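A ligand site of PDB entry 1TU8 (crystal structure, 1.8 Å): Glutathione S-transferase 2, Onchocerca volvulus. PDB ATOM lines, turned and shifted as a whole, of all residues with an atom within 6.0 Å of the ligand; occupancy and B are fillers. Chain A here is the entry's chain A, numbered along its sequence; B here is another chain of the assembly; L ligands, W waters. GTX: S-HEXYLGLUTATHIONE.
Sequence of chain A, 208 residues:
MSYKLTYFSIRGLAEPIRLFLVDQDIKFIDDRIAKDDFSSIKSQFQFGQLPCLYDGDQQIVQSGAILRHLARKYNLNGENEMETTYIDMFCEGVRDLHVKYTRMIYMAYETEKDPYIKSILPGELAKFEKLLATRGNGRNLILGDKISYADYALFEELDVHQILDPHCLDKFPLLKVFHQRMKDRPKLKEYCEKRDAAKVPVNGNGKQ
N of Ser 63 lies within hydrogen-bond range of O12 of the ligand.
O11 of the ligand sits at hydrogen-bond distance from OG of Ser 63, at 2.6 Å.
O2 of the ligand lies within hydrogen-bond range of N of Leu 50 (2.9 Å).
The backbone carbonyl oxygen (O) of Leu 50 sits at hydrogen-bond distance from a nitrogen (N2) of the ligand (2.8 Å).
The side-chain carboxylate of Asp 96 of chain B lies within salt-bridge range of a nitrogen (N1) of the ligand (2.9 Å).
N1 of the ligand lies close to NE2 of Gln 62 (3.0 Å).
An oxygen (O32) of the ligand sits close to the side-chain amide oxygen (OE1) of Gln 49, at 3.0 Å.
OH of Tyr 7 sits close to SG2 of the ligand.
The guanidinium group (NH2) of Arg 95 is in salt-bridge range of an oxygen (O11) of the ligand (3.2 Å).
NZ of Lys 42 is in salt-bridge range of O31 of the ligand (3.4 Å).
The side-chain hydroxyl (OG) of Ser 63 lies within hydrogen-bond range of the guanidinium group (NH1) of Arg 95 (2.9 Å).
OE1 of Gln 62 sits close to OD2 of Asp 96 of chain B.
The side-chain hydroxyl of Tyr 7 sits at hydrogen-bond distance from the backbone NH of Leu 13, at 3.1 Å.
OH of Tyr 106 sits at hydrogen-bond distance from N of Gly 204 (2.8 Å).
NZ of Lys 42 sits at hydrogen-bond distance from O of Gly 48, 2.7 Å away.
Phe 8 touches the ligand.
Ile 10 touches the ligand.
CD1 of Leu 13 touches SG2 of the ligand, 3.6 Å away.
Phe 38 touches the ligand (CE2 to O31, 3.5 Å).
Pro 51 touches the ligand.
OH of Tyr 106 touches C4S of the ligand, at 3.3 Å.
Gly 204 touches the ligand.
Hydrophobic or aromatic side chains within 4 Å of the ligand: Tyr 7, Phe 8, Ile 10, Leu 13, Phe 38 and Pro 51.
15 residues have an atom within 4 Å of the ligand: Tyr 7, Phe 8, Ile 10, Leu 13, Phe 38, Lys 42, Gln 49, Leu 50, Pro 51, Gln 62, Ser 63, Arg 95, Tyr 106, Gly 204 and Asp 96 of chain B.
Water W2 lies within hydrogen-bond range of O12 of the ligand (2.7 Å), O of Pro 51 (2.8 Å) and N of Gln 62 (3.0 Å).
Water W5 lies within hydrogen-bond range of the side-chain carboxylate of Glu 92 of chain B, a nitrogen (N1) of the ligand, the side-chain carboxylate of Asp 96 of chain B and the side-chain amide nitrogen of Gln 62.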
ATOM      1  N   TYR A   7       1.440  -3.447 -12.440  1.00  0.00           N
ATOM      2  CA  TYR A   7       1.099  -2.093 -12.011  1.00  0.00           C
ATOM      3  C   TYR A   7       0.524  -1.320 -13.190  1.00  0.00           C
ATOM      4  O   TYR A   7       0.446  -1.825 -14.311  1.00  0.00           O
ATOM      5  CB  TYR A   7       2.344  -1.388 -11.463  1.00  0.00           C
ATOM      6  CG  TYR A   7       2.061  -0.083 -10.732  1.00  0.00           C
ATOM      7  CD1 TYR A   7       2.632   1.108 -11.172  1.00  0.00           C
ATOM      8  CD2 TYR A   7       1.251  -0.044  -9.597  1.00  0.00           C
ATOM      9  CE1 TYR A   7       2.393   2.309 -10.507  1.00  0.00           C
ATOM     10  CE2 TYR A   7       1.002   1.157  -8.921  1.00  0.00           C
ATOM     11  CZ  TYR A   7       1.583   2.328  -9.391  1.00  0.00           C
ATOM     12  OH  TYR A   7       1.370   3.522  -8.750  1.00  0.00           O
ATOM     13  N   PHE A   8       0.095  -0.092 -12.926  1.00  0.00           N
ATOM     14  CA  PHE A   8      -0.353   0.817 -13.972  1.00  0.00           C
ATOM     15  C   PHE A   8       0.826   1.274 -14.817  1.00  0.00           C
ATOM     16  O   PHE A   8       1.984   1.080 -14.453  1.00  0.00           O
ATOM     17  CB  PHE A   8      -1.106   1.995 -13.332  1.00  0.00           C
ATOM     18  CG  PHE A   8      -2.359   1.565 -12.656  1.00  0.00           C
ATOM     19  CD1 PHE A   8      -2.396   1.398 -11.274  1.00  0.00           C
ATOM     20  CD2 PHE A   8      -3.497   1.246 -13.396  1.00  0.00           C
ATOM     21  CE1 PHE A   8      -3.556   0.965 -10.645  1.00  0.00           C
ATOM     22  CE2 PHE A   8      -4.650   0.807 -12.771  1.00  0.00           C
ATOM     23  CZ  PHE A   8      -4.674   0.666 -11.386  1.00  0.00           C
ATOM     24  N   ILE A  10       2.559   3.771 -15.371  1.00  0.00           N
ATOM     25  CA  ILE A  10       3.171   4.985 -14.855  1.00  0.00           C
ATOM     26  C   ILE A  10       4.339   4.576 -13.959  1.00  0.00           C
ATOM     27  O   ILE A  10       4.519   3.398 -13.656  1.00  0.00           O
ATOM     28  CB  ILE A  10       2.141   5.806 -14.031  1.00  0.00           C
ATOM     29  CG1 ILE A  10       1.778   5.065 -12.729  1.00  0.00           C
ATOM     30  CG2 ILE A  10       0.866   6.065 -14.845  1.00  0.00           C
ATOM     31  CD1 ILE A  10       0.930   5.899 -11.777  1.00  0.00           C
ATOM     32  N   GLY A  12       4.985   5.977 -10.531  1.00  0.00           N
ATOM     33  CA  GLY A  12       4.212   5.814  -9.311  1.00  0.00           C
ATOM     34  C   GLY A  12       4.933   5.015  -8.237  1.00  0.00           C
ATOM     35  O   GLY A  12       6.148   5.126  -8.063  1.00  0.00           O
ATOM     36  N   LEU A  13       4.175   4.150  -7.564  1.00  0.00           N
ATOM     37  CA  LEU A  13       4.667   3.329  -6.457  1.00  0.00           C
ATOM     38  C   LEU A  13       5.546   2.161  -6.895  1.00  0.00           C
ATOM     39  O   LEU A  13       6.271   1.589  -6.083  1.00  0.00           O
ATOM     40  CB  LEU A  13       3.474   2.744  -5.683  1.00  0.00           C
ATOM     41  CG  LEU A  13       2.562   3.695  -4.912  1.00  0.00           C
ATOM     42  CD1 LEU A  13       1.471   2.901  -4.208  1.00  0.00           C
ATOM     43  CD2 LEU A  13       3.369   4.514  -3.912  1.00  0.00           C
ATOM     44  N   LYS A  35      -5.684   1.472 -17.323  1.00  0.00           N
ATOM     45  CA  LYS A  35      -6.558   1.830 -16.200  1.00  0.00           C
ATOM     46  C   LYS A  35      -7.943   1.194 -16.304  1.00  0.00           C
ATOM     47  O   LYS A  35      -8.508   0.802 -15.285  1.00  0.00           O
ATOM     48  CB  LYS A  35      -6.687   3.373 -16.137  1.00  0.00           C
ATOM     49  CG  LYS A  35      -5.450   4.248 -16.237  1.00  0.00           C
ATOM     50  CD  LYS A  35      -5.775   5.745 -16.207  1.00  0.00           C
ATOM     51  CE  LYS A  35      -4.529   6.621 -16.318  1.00  0.00           C
ATOM     52  NZ  LYS A  35      -4.830   8.055 -16.264  1.00  0.00           N
ATOM     53  N   PHE A  38      -8.330  -2.545 -15.084  1.00  0.00           N
ATOM     54  CA  PHE A  38      -8.135  -2.909 -13.683  1.00  0.00           C
ATOM     55  C   PHE A  38      -9.417  -3.339 -12.977  1.00  0.00           C
ATOM     56  O   PHE A  38      -9.382  -4.234 -12.125  1.00  0.00           O
ATOM     57  CB  PHE A  38      -7.455  -1.804 -12.874  1.00  0.00           C
ATOM     58  CG  PHE A  38      -7.119  -2.247 -11.484  1.00  0.00           C
ATOM     59  CD1 PHE A  38      -6.235  -3.296 -11.287  1.00  0.00           C
ATOM     60  CD2 PHE A  38      -7.745  -1.676 -10.377  1.00  0.00           C
ATOM     61  CE1 PHE A  38      -5.948  -3.744 -10.013  1.00  0.00           C
ATOM     62  CE2 PHE A  38      -7.448  -2.114  -9.104  1.00  0.00           C
ATOM     63  CZ  PHE A  38      -6.551  -3.146  -8.914  1.00  0.00           C
ATOM     64  N   LYS A  42      -9.647  -6.613 -10.344  1.00  0.00           N
ATOM     65  CA  LYS A  42      -9.431  -5.991  -9.030  1.00  0.00           C
ATOM     66  C   LYS A  42      -9.507  -6.967  -7.852  1.00  0.00           C
ATOM     67  O   LYS A  42      -8.673  -6.920  -6.945  1.00  0.00           O
ATOM     68  CB  LYS A  42     -10.410  -4.819  -8.827  1.00  0.00           C
ATOM     69  CG  LYS A  42     -10.429  -4.223  -7.425  1.00  0.00           C
ATOM     70  CD  LYS A  42     -11.093  -2.839  -7.399  1.00  0.00           C
ATOM     71  CE  LYS A  42     -11.124  -2.249  -5.981  1.00  0.00           C
ATOM     72  NZ  LYS A  42      -9.911  -1.420  -5.650  1.00  0.00           N
ATOM     73  N   GLY A  48      -7.239  -5.205  -3.226  1.00  0.00           N
ATOM     74  CA  GLY A  48      -7.876  -4.620  -4.395  1.00  0.00           C
ATOM     75  C   GLY A  48      -7.044  -3.561  -5.095  1.00  0.00           C
ATOM     76  O   GLY A  48      -7.586  -2.690  -5.779  1.00  0.00           O
ATOM     77  N   GLN A  49      -5.720  -3.636  -4.934  1.00  0.00           N
ATOM     78  CA  GLN A  49      -4.821  -2.588  -5.421  1.00  0.00           C
ATOM     79  C   GLN A  49      -3.500  -3.142  -5.922  1.00  0.00           C
ATOM     80  O   GLN A  49      -3.134  -4.275  -5.636  1.00  0.00           O
ATOM     81  CB  GLN A  49      -4.572  -1.557  -4.311  1.00  0.00           C
ATOM     82  CG  GLN A  49      -5.784  -0.680  -4.018  1.00  0.00           C
ATOM     83  CD  GLN A  49      -5.444   0.636  -3.353  1.00  0.00           C
ATOM     84  OE1 GLN A  49      -5.921   1.697  -3.777  1.00  0.00           O
ATOM     85  NE2 GLN A  49      -4.638   0.585  -2.304  1.00  0.00           N
ATOM     86  N   LEU A  50      -2.796  -2.295  -6.667  1.00  0.00           N
ATOM     87  CA  LEU A  50      -1.488  -2.580  -7.251  1.00  0.00           C
ATOM     88  C   LEU A  50      -0.466  -1.607  -6.662  1.00  0.00           C
ATOM     89  O   LEU A  50      -0.870  -0.546  -6.166  1.00  0.00           O
ATOM     90  CB  LEU A  50      -1.569  -2.409  -8.758  1.00  0.00           C
ATOM     91  CG  LEU A  50      -2.595  -3.284  -9.488  1.00  0.00           C
ATOM     92  CD1 LEU A  50      -2.590  -2.948 -10.971  1.00  0.00           C
ATOM     93  CD2 LEU A  50      -2.303  -4.762  -9.264  1.00  0.00           C
ATOM     94  N   PRO A  51       0.840  -1.897  -6.705  1.00  0.00           N
ATOM     95  CA  PRO A  51       1.464  -3.031  -7.420  1.00  0.00           C
ATOM     96  C   PRO A  51       1.331  -4.420  -6.791  1.00  0.00           C
ATOM     97  O   PRO A  51       1.027  -4.558  -5.608  1.00  0.00           O
ATOM     98  CB  PRO A  51       2.940  -2.626  -7.456  1.00  0.00           C
ATOM     99  CG  PRO A  51       3.130  -1.792  -6.197  1.00  0.00           C
ATOM    100  CD  PRO A  51       1.841  -1.050  -6.028  1.00  0.00           C
ATOM    101  N   VAL A  61       1.346  -8.274  -2.679  1.00  0.00           N
ATOM    102  CA  VAL A  61       0.962  -6.882  -2.854  1.00  0.00           C
ATOM    103  C   VAL A  61       1.617  -6.041  -1.755  1.00  0.00           C
ATOM    104  O   VAL A  61       2.299  -6.579  -0.886  1.00  0.00           O
ATOM    105  CB  VAL A  61      -0.577  -6.682  -2.860  1.00  0.00           C
ATOM    106  CG1 VAL A  61      -1.205  -7.354  -4.090  1.00  0.00           C
ATOM    107  CG2 VAL A  61      -1.216  -7.193  -1.578  1.00  0.00           C
ATOM    108  N   GLN A  62       1.418  -4.721  -1.868  1.00  0.00           N
ATOM    109  CA  GLN A  62       1.964  -3.710  -0.963  1.00  0.00           C
ATOM    110  C   GLN A  62       3.416  -3.388  -1.328  1.00  0.00           C
ATOM    111  O   GLN A  62       4.321  -4.190  -1.070  1.00  0.00           O
ATOM    112  CB  GLN A  62       1.814  -4.090   0.527  1.00  0.00           C
ATOM    113  CG  GLN A  62       0.384  -4.074   1.041  1.00  0.00           C
ATOM    114  CD  GLN A  62      -0.208  -2.668   1.196  1.00  0.00           C
ATOM    115  OE1 GLN A  62      -1.409  -2.525   1.439  1.00  0.00           O
ATOM    116  NE2 GLN A  62       0.626  -1.658   1.040  1.00  0.00           N
ATOM    117  N   SER A  63       3.621  -2.219  -1.946  1.00  0.00           N
ATOM    118  CA  SER A  63       4.913  -1.834  -2.485  1.00  0.00           C
ATOM    119  C   SER A  63       6.062  -1.925  -1.478  1.00  0.00           C
ATOM    120  O   SER A  63       7.158  -2.324  -1.844  1.00  0.00           O
ATOM    121  CB  SER A  63       4.863  -0.423  -3.075  1.00  0.00           C
ATOM    122  OG  SER A  63       4.520   0.550  -2.106  1.00  0.00           O
ATOM    123  N   GLY A  64       5.833  -1.522  -0.232  1.00  0.00           N
ATOM    124  CA  GLY A  64       6.870  -1.611   0.784  1.00  0.00           C
ATOM    125  C   GLY A  64       7.220  -3.034   1.163  1.00  0.00           C
ATOM    126  O   GLY A  64       8.383  -3.346   1.385  1.00  0.00           O
ATOM    127  N   ARG A  95       8.960   7.430   1.684  1.00  0.00           N
ATOM    128  CA  ARG A  95       7.532   7.230   1.470  1.00  0.00           C
ATOM    129  C   ARG A  95       6.661   8.393   1.995  1.00  0.00           C
ATOM    130  O   ARG A  95       5.671   8.753   1.370  1.00  0.00           O
ATOM    131  CB  ARG A  95       7.078   5.918   2.114  1.00  0.00           C
ATOM    132  CG  ARG A  95       7.658   4.691   1.464  1.00  0.00           C
ATOM    133  CD  ARG A  95       7.130   3.411   2.074  1.00  0.00           C
ATOM    134  NE  ARG A  95       5.685   3.298   1.893  1.00  0.00           N
ATOM    135  CZ  ARG A  95       5.093   2.509   0.993  1.00  0.00           C
ATOM    136  NH1 ARG A  95       5.812   1.765   0.173  1.00  0.00           N
ATOM    137  NH2 ARG A  95       3.769   2.478   0.920  1.00  0.00           N
ATOM    138  N   TYR A 106      -2.320  14.837  -7.143  1.00  0.00           N
ATOM    139  CA  TYR A 106      -3.659  14.310  -7.428  1.00  0.00           C
ATOM    140  C   TYR A 106      -4.824  15.176  -6.933  1.00  0.00           C
ATOM    141  O   TYR A 106      -5.919  15.116  -7.503  1.00  0.00           O
ATOM    142  CB  TYR A 106      -3.803  12.891  -6.849  1.00  0.00           C
ATOM    143  CG  TYR A 106      -3.040  11.848  -7.647  1.00  0.00           C
ATOM    144  CD1 TYR A 106      -1.799  11.375  -7.220  1.00  0.00           C
ATOM    145  CD2 TYR A 106      -3.559  11.337  -8.831  1.00  0.00           C
ATOM    146  CE1 TYR A 106      -1.110  10.425  -7.931  1.00  0.00           C
ATOM    147  CE2 TYR A 106      -2.871  10.397  -9.562  1.00  0.00           C
ATOM    148  CZ  TYR A 106      -1.639   9.945  -9.106  1.00  0.00           C
ATOM    149  OH  TYR A 106      -0.940   9.005  -9.817  1.00  0.00           O
ATOM    150  N   ASN A 203       2.923  10.015 -13.014  1.00  0.00           N
ATOM    151  CA  ASN A 203       1.668   9.875 -12.291  1.00  0.00           C
ATOM    152  C   ASN A 203       0.498   9.544 -13.221  1.00  0.00           C
ATOM    153  O   ASN A 203       0.635   9.597 -14.447  1.00  0.00           O
ATOM    154  CB  ASN A 203       1.396  11.170 -11.520  1.00  0.00           C
ATOM    155  CG  ASN A 203       2.578  11.597 -10.668  1.00  0.00           C
ATOM    156  OD1 ASN A 203       3.181  12.655 -10.871  1.00  0.00           O
ATOM    157  ND2 ASN A 203       2.935  10.747  -9.711  1.00  0.00           N
ATOM    158  N   GLY A 204      -0.637   9.174 -12.637  1.00  0.00           N
ATOM    159  CA  GLY A 204      -1.766   8.678 -13.399  1.00  0.00           C
ATOM    160  C   GLY A 204      -2.683   9.740 -13.982  1.00  0.00           C
ATOM    161  O   GLY A 204      -3.591   9.413 -14.756  1.00  0.00           O
ATOM    162  N   ASN A 205      -2.477  10.992 -13.604  1.00  0.00           N
ATOM    163  CA  ASN A 205      -3.358  12.092 -14.015  1.00  0.00           C
ATOM    164  C   ASN A 205      -2.679  13.037 -15.002  1.00  0.00           C
ATOM    165  O   ASN A 205      -3.191  14.125 -15.281  1.00  0.00           O
ATOM    166  CB  ASN A 205      -3.854  12.866 -12.782  1.00  0.00           C
ATOM    167  CG  ASN A 205      -2.752  13.664 -12.106  1.00  0.00           C
ATOM    168  OD1 ASN A 205      -1.579  13.517 -12.426  1.00  0.00           O
ATOM    169  ND2 ASN A 205      -3.127  14.510 -11.159  1.00  0.00           N
ATOM    170  N   GLU B  92       0.975  -3.603   6.305  1.00  0.00           N
ATOM    171  CA  GLU B  92       0.899  -2.463   5.395  1.00  0.00           C
ATOM    172  C   GLU B  92      -0.560  -2.202   4.984  1.00  0.00           C
ATOM    173  O   GLU B  92      -0.941  -1.061   4.802  1.00  0.00           O
ATOM    174  CB  GLU B  92       1.767  -2.679   4.157  1.00  0.00           C
ATOM    175  CG  GLU B  92       3.260  -2.590   4.454  1.00  0.00           C
ATOM    176  CD  GLU B  92       3.668  -1.179   4.831  1.00  0.00           C
ATOM    177  OE1 GLU B  92       3.593  -0.295   3.950  1.00  0.00           O
ATOM    178  OE2 GLU B  92       4.047  -0.957   6.007  1.00  0.00           O
ATOM    179  N   ASP B  96      -2.798   1.300   5.523  1.00  0.00           N
ATOM    180  CA  ASP B  96      -3.660   1.901   4.499  1.00  0.00           C
ATOM    181  C   ASP B  96      -5.029   2.266   5.073  1.00  0.00           C
ATOM    182  O   ASP B  96      -5.571   3.314   4.754  1.00  0.00           O
ATOM    183  CB  ASP B  96      -3.858   0.948   3.311  1.00  0.00           C
ATOM    184  CG  ASP B  96      -2.723   1.000   2.314  1.00  0.00           C
ATOM    185  OD1 ASP B  96      -2.001   2.014   2.257  1.00  0.00           O
ATOM    186  OD2 ASP B  96      -2.492   0.071   1.513  1.00  0.00           O
HETATM  187  N1  GTX L   1      -0.064   1.118   0.263  1.00  0.00           N
HETATM  188  CA1 GTX L   1      -0.268   0.523  -1.048  1.00  0.00           C
HETATM  189  C1  GTX L   1       1.074   0.195  -1.628  1.00  0.00           C
HETATM  190  O11 GTX L   1       2.113   0.860  -1.230  1.00  0.00           O
HETATM  191  O12 GTX L   1       1.223  -0.726  -2.548  1.00  0.00           O
HETATM  192  CB1 GTX L   1      -1.034   1.520  -1.920  1.00  0.00           C
HETATM  193  CG1 GTX L   1      -1.517   0.882  -3.227  1.00  0.00           C
HETATM  194  CD1 GTX L   1      -2.257   1.883  -4.083  1.00  0.00           C
HETATM  195  OE1 GTX L   1      -2.632   3.124  -3.559  1.00  0.00           O
HETATM  196  N2  GTX L   1      -2.555   1.501  -5.318  1.00  0.00           N
HETATM  197  CA2 GTX L   1      -3.285   2.301  -6.292  1.00  0.00           C
HETATM  198  C2  GTX L   1      -4.396   1.513  -6.918  1.00  0.00           C
HETATM  199  O2  GTX L   1      -4.236   0.142  -7.167  1.00  0.00           O
HETATM  200  CB2 GTX L   1      -2.326   2.740  -7.391  1.00  0.00           C
HETATM  201  SG2 GTX L   1      -0.983   3.747  -6.737  1.00  0.00           S
HETATM  202  C1S GTX L   1      -1.859   5.323  -6.946  1.00  0.00           C
HETATM  203  C2S GTX L   1      -1.559   6.006  -8.291  1.00  0.00           C
HETATM  204  C3S GTX L   1      -2.340   5.347  -9.433  1.00  0.00           C
HETATM  205  C4S GTX L   1      -2.647   6.303 -10.588  1.00  0.00           C
HETATM  206  C5S GTX L   1      -3.389   5.557 -11.693  1.00  0.00           C
HETATM  207  C6S GTX L   1      -4.827   5.233 -11.296  1.00  0.00           C
HETATM  208  N3  GTX L   1      -5.511   2.162  -7.201  1.00  0.00           N
HETATM  209  CA3 GTX L   1      -6.524   1.579  -8.067  1.00  0.00           C
HETATM  210  C3  GTX L   1      -7.794   1.287  -7.309  1.00  0.00           C
HETATM  211  O31 GTX L   1      -8.842   0.823  -7.942  1.00  0.00           O
HETATM  212  O32 GTX L   1      -7.873   1.485  -6.016  1.00  0.00           O
HETATM  213  O   HOH W   1      -5.792   4.925  -6.281  1.00  0.00           O
HETATM  214  O   HOH W   2      -0.058  -2.844  -3.625  1.00  0.00           O
HETATM  215  O   HOH W   3       0.615   3.803   0.036  1.00  0.00           O
HETATM  216  O   HOH W   4       3.428  -0.958   1.365  1.00  0.00           O
HETATM  217  O   HOH W   5       0.862   0.856   3.182  1.00  0.00           O
HETATM  218  O   HOH W   6      -1.378   4.982  -2.439  1.00  0.00           O
